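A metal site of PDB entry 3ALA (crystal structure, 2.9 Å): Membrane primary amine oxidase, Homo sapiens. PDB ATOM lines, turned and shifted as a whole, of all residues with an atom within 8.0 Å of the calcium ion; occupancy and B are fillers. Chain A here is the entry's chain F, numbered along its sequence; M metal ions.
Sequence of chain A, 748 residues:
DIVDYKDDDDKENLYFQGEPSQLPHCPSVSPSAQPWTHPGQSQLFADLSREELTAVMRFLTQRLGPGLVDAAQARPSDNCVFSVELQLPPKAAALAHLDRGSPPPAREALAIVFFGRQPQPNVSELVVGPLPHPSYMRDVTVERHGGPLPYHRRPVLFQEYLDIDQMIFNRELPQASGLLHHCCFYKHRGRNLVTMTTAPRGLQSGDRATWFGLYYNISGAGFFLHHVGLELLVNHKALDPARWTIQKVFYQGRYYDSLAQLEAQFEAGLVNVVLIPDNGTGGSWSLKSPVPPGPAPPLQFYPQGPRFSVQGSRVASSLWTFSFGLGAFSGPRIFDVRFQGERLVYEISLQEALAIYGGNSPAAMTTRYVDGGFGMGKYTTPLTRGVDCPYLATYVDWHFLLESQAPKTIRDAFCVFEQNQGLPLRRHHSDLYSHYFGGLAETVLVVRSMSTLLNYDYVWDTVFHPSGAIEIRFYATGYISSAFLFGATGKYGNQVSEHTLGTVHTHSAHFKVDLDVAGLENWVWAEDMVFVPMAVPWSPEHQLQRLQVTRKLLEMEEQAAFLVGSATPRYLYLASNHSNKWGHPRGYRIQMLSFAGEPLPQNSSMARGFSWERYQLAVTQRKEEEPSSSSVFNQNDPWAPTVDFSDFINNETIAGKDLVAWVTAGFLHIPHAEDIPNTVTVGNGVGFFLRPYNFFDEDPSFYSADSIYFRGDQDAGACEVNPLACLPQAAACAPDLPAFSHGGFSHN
Lys 91 touches the calcium ion (NZ to CA, 3.6 Å). The nearest printed residue that does not touch the calcium ion is Leu 520 (4.3 Å).
The calcium ion is bound by OD1 of Asp 516, O of Leu 515, OD1 of Asp 658, OD1 of Asp 514 and O of Leu 659.
N of Asp 514 is in hydrogen-bond range of O of Glu 347 (2.8 Å). The backbone NH (N) of Asp 516 lies within hydrogen-bond range of the backbone carbonyl oxygen (O) of Leu 344. The side-chain carboxylate of Asp 514 lies within salt-bridge range of the side-chain amino group of Lys 91 (2.7 Å). The side-chain amino group of Lys 91 sits close to the side-chain carboxylate of Asp 658 (3.1 Å). OD2 of Asp 516 is in salt-bridge range of NZ of Lys 91, 3.2 Å away. The backbone carbonyl oxygen (O) of Asp 514 is in hydrogen-bond range of the backbone NH (N) of Tyr 346, at 3.0 Å. The side-chain carboxylate (OD2) of Asp 514 is in salt-bridge range of the guanidinium group (NE) of Arg 622, 3.4 Å away. The backbone carbonyl oxygen (O) of Asp 658 lies within hydrogen-bond range of the backbone NH (N) of Arg 622, 2.7 Å away.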
ATOM      1  N   LYS A  91      -4.586  11.462 -30.030  1.00  0.00           N
ATOM      2  CA  LYS A  91      -4.117  10.101 -29.845  1.00  0.00           C
ATOM      3  C   LYS A  91      -5.299   9.150 -29.782  1.00  0.00           C
ATOM      4  O   LYS A  91      -5.283   8.125 -30.482  1.00  0.00           O
ATOM      5  CB  LYS A  91      -3.285   9.936 -28.574  1.00  0.00           C
ATOM      6  CG  LYS A  91      -2.187   8.875 -28.757  1.00  0.00           C
ATOM      7  CD  LYS A  91      -1.861   8.044 -27.493  1.00  0.00           C
ATOM      8  CE  LYS A  91      -0.805   8.720 -26.622  1.00  0.00           C
ATOM      9  NZ  LYS A  91      -0.012   7.800 -25.772  1.00  0.00           N
ATOM     10  N   LEU A 344       5.456  -0.445 -29.405  1.00  0.00           N
ATOM     11  CA  LEU A 344       6.279  -0.040 -28.276  1.00  0.00           C
ATOM     12  C   LEU A 344       6.095   1.448 -27.974  1.00  0.00           C
ATOM     13  O   LEU A 344       5.904   1.870 -26.823  1.00  0.00           O
ATOM     14  CB  LEU A 344       7.746  -0.287 -28.576  1.00  0.00           C
ATOM     15  CG  LEU A 344       8.133  -1.747 -28.840  1.00  0.00           C
ATOM     16  CD1 LEU A 344       9.645  -1.855 -29.215  1.00  0.00           C
ATOM     17  CD2 LEU A 344       7.835  -2.624 -27.608  1.00  0.00           C
ATOM     18  N   VAL A 345       6.135   2.248 -29.022  1.00  0.00           N
ATOM     19  CA  VAL A 345       6.028   3.685 -28.895  1.00  0.00           C
ATOM     20  C   VAL A 345       4.941   4.225 -29.820  1.00  0.00           C
ATOM     21  O   VAL A 345       4.836   3.788 -30.976  1.00  0.00           O
ATOM     22  CB  VAL A 345       7.376   4.366 -29.185  1.00  0.00           C
ATOM     23  CG1 VAL A 345       8.445   3.408 -29.717  1.00  0.00           C
ATOM     24  CG2 VAL A 345       7.193   5.723 -29.800  1.00  0.00           C
ATOM     25  N   TYR A 346       4.125   5.148 -29.292  1.00  0.00           N
ATOM     26  CA  TYR A 346       3.212   5.917 -30.108  1.00  0.00           C
ATOM     27  C   TYR A 346       3.983   7.004 -30.858  1.00  0.00           C
ATOM     28  O   TYR A 346       3.704   7.259 -32.030  1.00  0.00           O
ATOM     29  CB  TYR A 346       2.140   6.567 -29.269  1.00  0.00           C
ATOM     30  CG  TYR A 346       1.207   7.452 -30.031  1.00  0.00           C
ATOM     31  CD1 TYR A 346       0.162   6.914 -30.743  1.00  0.00           C
ATOM     32  CD2 TYR A 346       1.350   8.826 -30.032  1.00  0.00           C
ATOM     33  CE1 TYR A 346      -0.728   7.707 -31.467  1.00  0.00           C
ATOM     34  CE2 TYR A 346       0.479   9.632 -30.721  1.00  0.00           C
ATOM     35  CZ  TYR A 346      -0.573   9.066 -31.442  1.00  0.00           C
ATOM     36  OH  TYR A 346      -1.465   9.847 -32.137  1.00  0.00           O
ATOM     37  N   GLU A 347       4.936   7.674 -30.198  1.00  0.00           N
ATOM     38  CA  GLU A 347       5.646   8.791 -30.805  1.00  0.00           C
ATOM     39  C   GLU A 347       7.055   8.982 -30.249  1.00  0.00           C
ATOM     40  O   GLU A 347       7.251   8.945 -29.052  1.00  0.00           O
ATOM     41  CB  GLU A 347       4.844  10.079 -30.592  1.00  0.00           C
ATOM     42  CG  GLU A 347       5.625  11.363 -31.012  1.00  0.00           C
ATOM     43  CD  GLU A 347       4.981  12.698 -30.525  1.00  0.00           C
ATOM     44  OE1 GLU A 347       3.839  12.645 -29.984  1.00  0.00           O
ATOM     45  OE2 GLU A 347       5.611  13.800 -30.727  1.00  0.00           O
ATOM     46  N   VAL A 513       9.379  11.223 -25.866  1.00  0.00           N
ATOM     47  CA  VAL A 513       9.350   9.785 -26.029  1.00  0.00           C
ATOM     48  C   VAL A 513       8.048   9.299 -25.414  1.00  0.00           C
ATOM     49  O   VAL A 513       7.978   9.136 -24.223  1.00  0.00           O
ATOM     50  CB  VAL A 513      10.551   9.128 -25.310  1.00  0.00           C
ATOM     51  CG1 VAL A 513      10.563   7.605 -25.531  1.00  0.00           C
ATOM     52  CG2 VAL A 513      11.859   9.747 -25.783  1.00  0.00           C
ATOM     53  N   ASP A 514       7.023   9.094 -26.226  1.00  0.00           N
ATOM     54  CA  ASP A 514       5.751   8.621 -25.706  1.00  0.00           C
ATOM     55  C   ASP A 514       5.658   7.102 -25.875  1.00  0.00           C
ATOM     56  O   ASP A 514       5.046   6.581 -26.825  1.00  0.00           O
ATOM     57  CB  ASP A 514       4.586   9.306 -26.395  1.00  0.00           C
ATOM     58  CG  ASP A 514       3.260   8.755 -25.929  1.00  0.00           C
ATOM     59  OD1 ASP A 514       3.237   7.940 -24.972  1.00  0.00           O
ATOM     60  OD2 ASP A 514       2.257   9.116 -26.544  1.00  0.00           O
ATOM     61  N   LEU A 515       6.288   6.392 -24.931  1.00  0.00           N
ATOM     62  CA  LEU A 515       6.187   4.943 -24.827  1.00  0.00           C
ATOM     63  C   LEU A 515       4.786   4.650 -24.395  1.00  0.00           C
ATOM     64  O   LEU A 515       4.187   5.421 -23.641  1.00  0.00           O
ATOM     65  CB  LEU A 515       7.155   4.410 -23.796  1.00  0.00           C
ATOM     66  CG  LEU A 515       8.587   4.183 -24.319  1.00  0.00           C
ATOM     67  CD1 LEU A 515       9.612   4.345 -23.196  1.00  0.00           C
ATOM     68  CD2 LEU A 515       8.721   2.814 -24.955  1.00  0.00           C
ATOM     69  N   ASP A 516       4.254   3.562 -24.944  1.00  0.00           N
ATOM     70  CA  ASP A 516       3.008   2.959 -24.476  1.00  0.00           C
ATOM     71  C   ASP A 516       3.242   1.475 -24.208  1.00  0.00           C
ATOM     72  O   ASP A 516       2.781   0.626 -24.985  1.00  0.00           O
ATOM     73  CB  ASP A 516       1.890   3.111 -25.522  1.00  0.00           C
ATOM     74  CG  ASP A 516       1.414   4.545 -25.676  1.00  0.00           C
ATOM     75  OD1 ASP A 516       1.782   5.424 -24.853  1.00  0.00           O
ATOM     76  OD2 ASP A 516       0.649   4.758 -26.623  1.00  0.00           O
ATOM     77  N   VAL A 517       3.915   1.174 -23.091  1.00  0.00           N
ATOM     78  CA  VAL A 517       4.436  -0.176 -22.862  1.00  0.00           C
ATOM     79  C   VAL A 517       3.256  -1.127 -22.624  1.00  0.00           C
ATOM     80  O   VAL A 517       2.515  -0.948 -21.665  1.00  0.00           O
ATOM     81  CB  VAL A 517       5.464  -0.251 -21.684  1.00  0.00           C
ATOM     82  CG1 VAL A 517       6.327  -1.552 -21.748  1.00  0.00           C
ATOM     83  CG2 VAL A 517       6.396   0.976 -21.694  1.00  0.00           C
ATOM     84  N   GLY A 519       0.285  -1.317 -23.823  1.00  0.00           N
ATOM     85  CA  GLY A 519      -0.928  -0.557 -23.532  1.00  0.00           C
ATOM     86  C   GLY A 519      -0.585   0.873 -23.117  1.00  0.00           C
ATOM     87  O   GLY A 519       0.605   1.236 -23.001  1.00  0.00           O
ATOM     88  N   LEU A 520      -1.614   1.671 -22.867  1.00  0.00           N
ATOM     89  CA  LEU A 520      -1.431   3.075 -22.441  1.00  0.00           C
ATOM     90  C   LEU A 520      -0.926   3.208 -20.980  1.00  0.00           C
ATOM     91  O   LEU A 520       0.111   3.868 -20.693  1.00  0.00           O
ATOM     92  CB  LEU A 520      -2.744   3.876 -22.553  1.00  0.00           C
ATOM     93  CG  LEU A 520      -3.257   4.293 -23.941  1.00  0.00           C
ATOM     94  CD1 LEU A 520      -4.419   5.237 -23.741  1.00  0.00           C
ATOM     95  CD2 LEU A 520      -2.112   4.943 -24.818  1.00  0.00           C
ATOM     96  N   GLU A 521      -1.676   2.588 -20.072  1.00  0.00           N
ATOM     97  CA  GLU A 521      -1.458   2.758 -18.652  1.00  0.00           C
ATOM     98  C   GLU A 521      -0.057   2.244 -18.327  1.00  0.00           C
ATOM     99  O   GLU A 521       0.255   1.053 -18.550  1.00  0.00           O
ATOM    100  CB  GLU A 521      -2.521   2.008 -17.836  1.00  0.00           C
ATOM    101  CG  GLU A 521      -3.894   2.697 -17.862  1.00  0.00           C
ATOM    102  CD  GLU A 521      -4.456   2.759 -19.268  1.00  0.00           C
ATOM    103  OE1 GLU A 521      -4.759   1.681 -19.808  1.00  0.00           O
ATOM    104  OE2 GLU A 521      -4.542   3.877 -19.837  1.00  0.00           O
ATOM    105  N   ASN A 522       0.765   3.154 -17.809  1.00  0.00           N
ATOM    106  CA  ASN A 522       2.111   2.804 -17.425  1.00  0.00           C
ATOM    107  C   ASN A 522       2.474   3.333 -16.022  1.00  0.00           C
ATOM    108  O   ASN A 522       1.786   4.182 -15.464  1.00  0.00           O
ATOM    109  CB  ASN A 522       3.087   3.273 -18.515  1.00  0.00           C
ATOM    110  CG  ASN A 522       3.016   2.422 -19.781  1.00  0.00           C
ATOM    111  OD1 ASN A 522       3.596   2.755 -20.793  1.00  0.00           O
ATOM    112  ND2 ASN A 522       2.317   1.288 -19.698  1.00  0.00           N
ATOM    113  N   LEU A 574       9.800   2.368 -17.670  1.00  0.00           N
ATOM    114  CA  LEU A 574       8.358   2.511 -17.695  1.00  0.00           C
ATOM    115  C   LEU A 574       7.754   1.153 -18.001  1.00  0.00           C
ATOM    116  O   LEU A 574       8.238   0.437 -18.891  1.00  0.00           O
ATOM    117  CB  LEU A 574       7.937   3.467 -18.800  1.00  0.00           C
ATOM    118  CG  LEU A 574       7.941   4.951 -18.434  1.00  0.00           C
ATOM    119  CD1 LEU A 574       9.376   5.350 -18.189  1.00  0.00           C
ATOM    120  CD2 LEU A 574       7.293   5.807 -19.528  1.00  0.00           C
ATOM    121  N   THR A 620       6.018  12.716 -17.429  1.00  0.00           N
ATOM    122  CA  THR A 620       4.801  13.459 -17.087  1.00  0.00           C
ATOM    123  C   THR A 620       3.598  12.776 -17.666  1.00  0.00           C
ATOM    124  O   THR A 620       3.721  11.942 -18.559  1.00  0.00           O
ATOM    125  CB  THR A 620       4.816  14.899 -17.697  1.00  0.00           C
ATOM    126  OG1 THR A 620       4.861  14.827 -19.132  1.00  0.00           O
ATOM    127  CG2 THR A 620       6.012  15.707 -17.184  1.00  0.00           C
ATOM    128  N   GLN A 621       2.431  13.124 -17.167  1.00  0.00           N
ATOM    129  CA  GLN A 621       1.215  12.633 -17.774  1.00  0.00           C
ATOM    130  C   GLN A 621       1.202  13.117 -19.215  1.00  0.00           C
ATOM    131  O   GLN A 621       1.534  14.281 -19.463  1.00  0.00           O
ATOM    132  CB  GLN A 621      -0.030  13.168 -17.070  1.00  0.00           C
ATOM    133  CG  GLN A 621      -0.363  12.475 -15.754  1.00  0.00           C
ATOM    134  CD  GLN A 621      -1.685  12.984 -15.150  1.00  0.00           C
ATOM    135  OE1 GLN A 621      -2.627  13.304 -15.893  1.00  0.00           O
ATOM    136  NE2 GLN A 621      -1.748  13.095 -13.809  1.00  0.00           N
ATOM    137  N   ARG A 622       0.842  12.260 -20.162  1.00  0.00           N
ATOM    138  CA  ARG A 622       0.637  12.730 -21.530  1.00  0.00           C
ATOM    139  C   ARG A 622      -0.712  13.426 -21.667  1.00  0.00           C
ATOM    140  O   ARG A 622      -1.710  12.936 -21.140  1.00  0.00           O
ATOM    141  CB  ARG A 622       0.680  11.606 -22.525  1.00  0.00           C
ATOM    142  CG  ARG A 622       0.709  12.139 -23.957  1.00  0.00           C
ATOM    143  CD  ARG A 622       0.064  11.153 -24.923  1.00  0.00           C
ATOM    144  NE  ARG A 622      -0.014  11.685 -26.281  1.00  0.00           N
ATOM    145  CZ  ARG A 622      -0.904  12.588 -26.703  1.00  0.00           C
ATOM    146  NH1 ARG A 622      -1.825  13.106 -25.868  1.00  0.00           N
ATOM    147  NH2 ARG A 622      -0.864  12.982 -27.965  1.00  0.00           N
ATOM    148  N   LYS A 657      -0.951   5.967 -15.710  1.00  0.00           N
ATOM    149  CA  LYS A 657      -1.541   6.828 -16.731  1.00  0.00           C
ATOM    150  C   LYS A 657      -0.813   6.630 -18.058  1.00  0.00           C
ATOM    151  O   LYS A 657       0.192   5.877 -18.156  1.00  0.00           O
ATOM    152  CB  LYS A 657      -1.424   8.282 -16.311  1.00  0.00           C
ATOM    153  CG  LYS A 657      -1.841   8.567 -14.898  1.00  0.00           C
ATOM    154  CD  LYS A 657      -3.322   8.311 -14.708  1.00  0.00           C
ATOM    155  CE  LYS A 657      -4.086   9.595 -14.375  1.00  0.00           C
ATOM    156  NZ  LYS A 657      -5.451   9.329 -13.722  1.00  0.00           N
ATOM    157  N   ASP A 658      -1.334   7.294 -19.088  1.00  0.00           N
ATOM    158  CA  ASP A 658      -0.574   7.425 -20.327  1.00  0.00           C
ATOM    159  C   ASP A 658       0.549   8.374 -20.054  1.00  0.00           C
ATOM    160  O   ASP A 658       0.344   9.578 -19.831  1.00  0.00           O
ATOM    161  CB  ASP A 658      -1.420   7.993 -21.460  1.00  0.00           C
ATOM    162  CG  ASP A 658      -0.656   8.035 -22.783  1.00  0.00           C
ATOM    163  OD1 ASP A 658       0.590   8.069 -22.790  1.00  0.00           O
ATOM    164  OD2 ASP A 658      -1.333   8.024 -23.812  1.00  0.00           O
ATOM    165  N   LEU A 659       1.748   7.828 -20.037  1.00  0.00           N
ATOM    166  CA  LEU A 659       2.918   8.612 -19.654  1.00  0.00           C
ATOM    167  C   LEU A 659       3.703   9.016 -20.901  1.00  0.00           C
ATOM    168  O   LEU A 659       3.507   8.485 -22.018  1.00  0.00           O
ATOM    169  CB  LEU A 659       3.804   7.778 -18.695  1.00  0.00           C
ATOM    170  CG  LEU A 659       3.183   7.375 -17.339  1.00  0.00           C
ATOM    171  CD1 LEU A 659       4.104   6.393 -16.575  1.00  0.00           C
ATOM    172  CD2 LEU A 659       2.858   8.618 -16.513  1.00  0.00           C
ATOM    173  N   VAL A 660       4.602   9.970 -20.687  1.00  0.00           N
ATOM    174  CA  VAL A 660       5.523  10.379 -21.715  1.00  0.00           C
ATOM    175  C   VAL A 660       6.789  10.865 -21.080  1.00  0.00           C
ATOM    176  O   VAL A 660       6.754  11.717 -20.209  1.00  0.00           O
ATOM    177  CB  VAL A 660       4.943  11.479 -22.577  1.00  0.00           C
ATOM    178  CG1 VAL A 660       4.328  12.588 -21.697  1.00  0.00           C
ATOM    179  CG2 VAL A 660       6.035  12.023 -23.544  1.00  0.00           C
ATOM    180  N   ALA A 661       7.916  10.337 -21.537  1.00  0.00           N
ATOM    181  CA  ALA A 661       9.219  10.721 -21.048  1.00  0.00           C
ATOM    182  C   ALA A 661       9.783  11.829 -21.913  1.00  0.00           C
ATOM    183  O   ALA A 661       9.559  11.860 -23.124  1.00  0.00           O
ATOM    184  CB  ALA A 661      10.137   9.520 -21.066  1.00  0.00           C
HETATM  185 CA    CA M   1       2.290   6.571 -23.251  1.00  0.00          CA
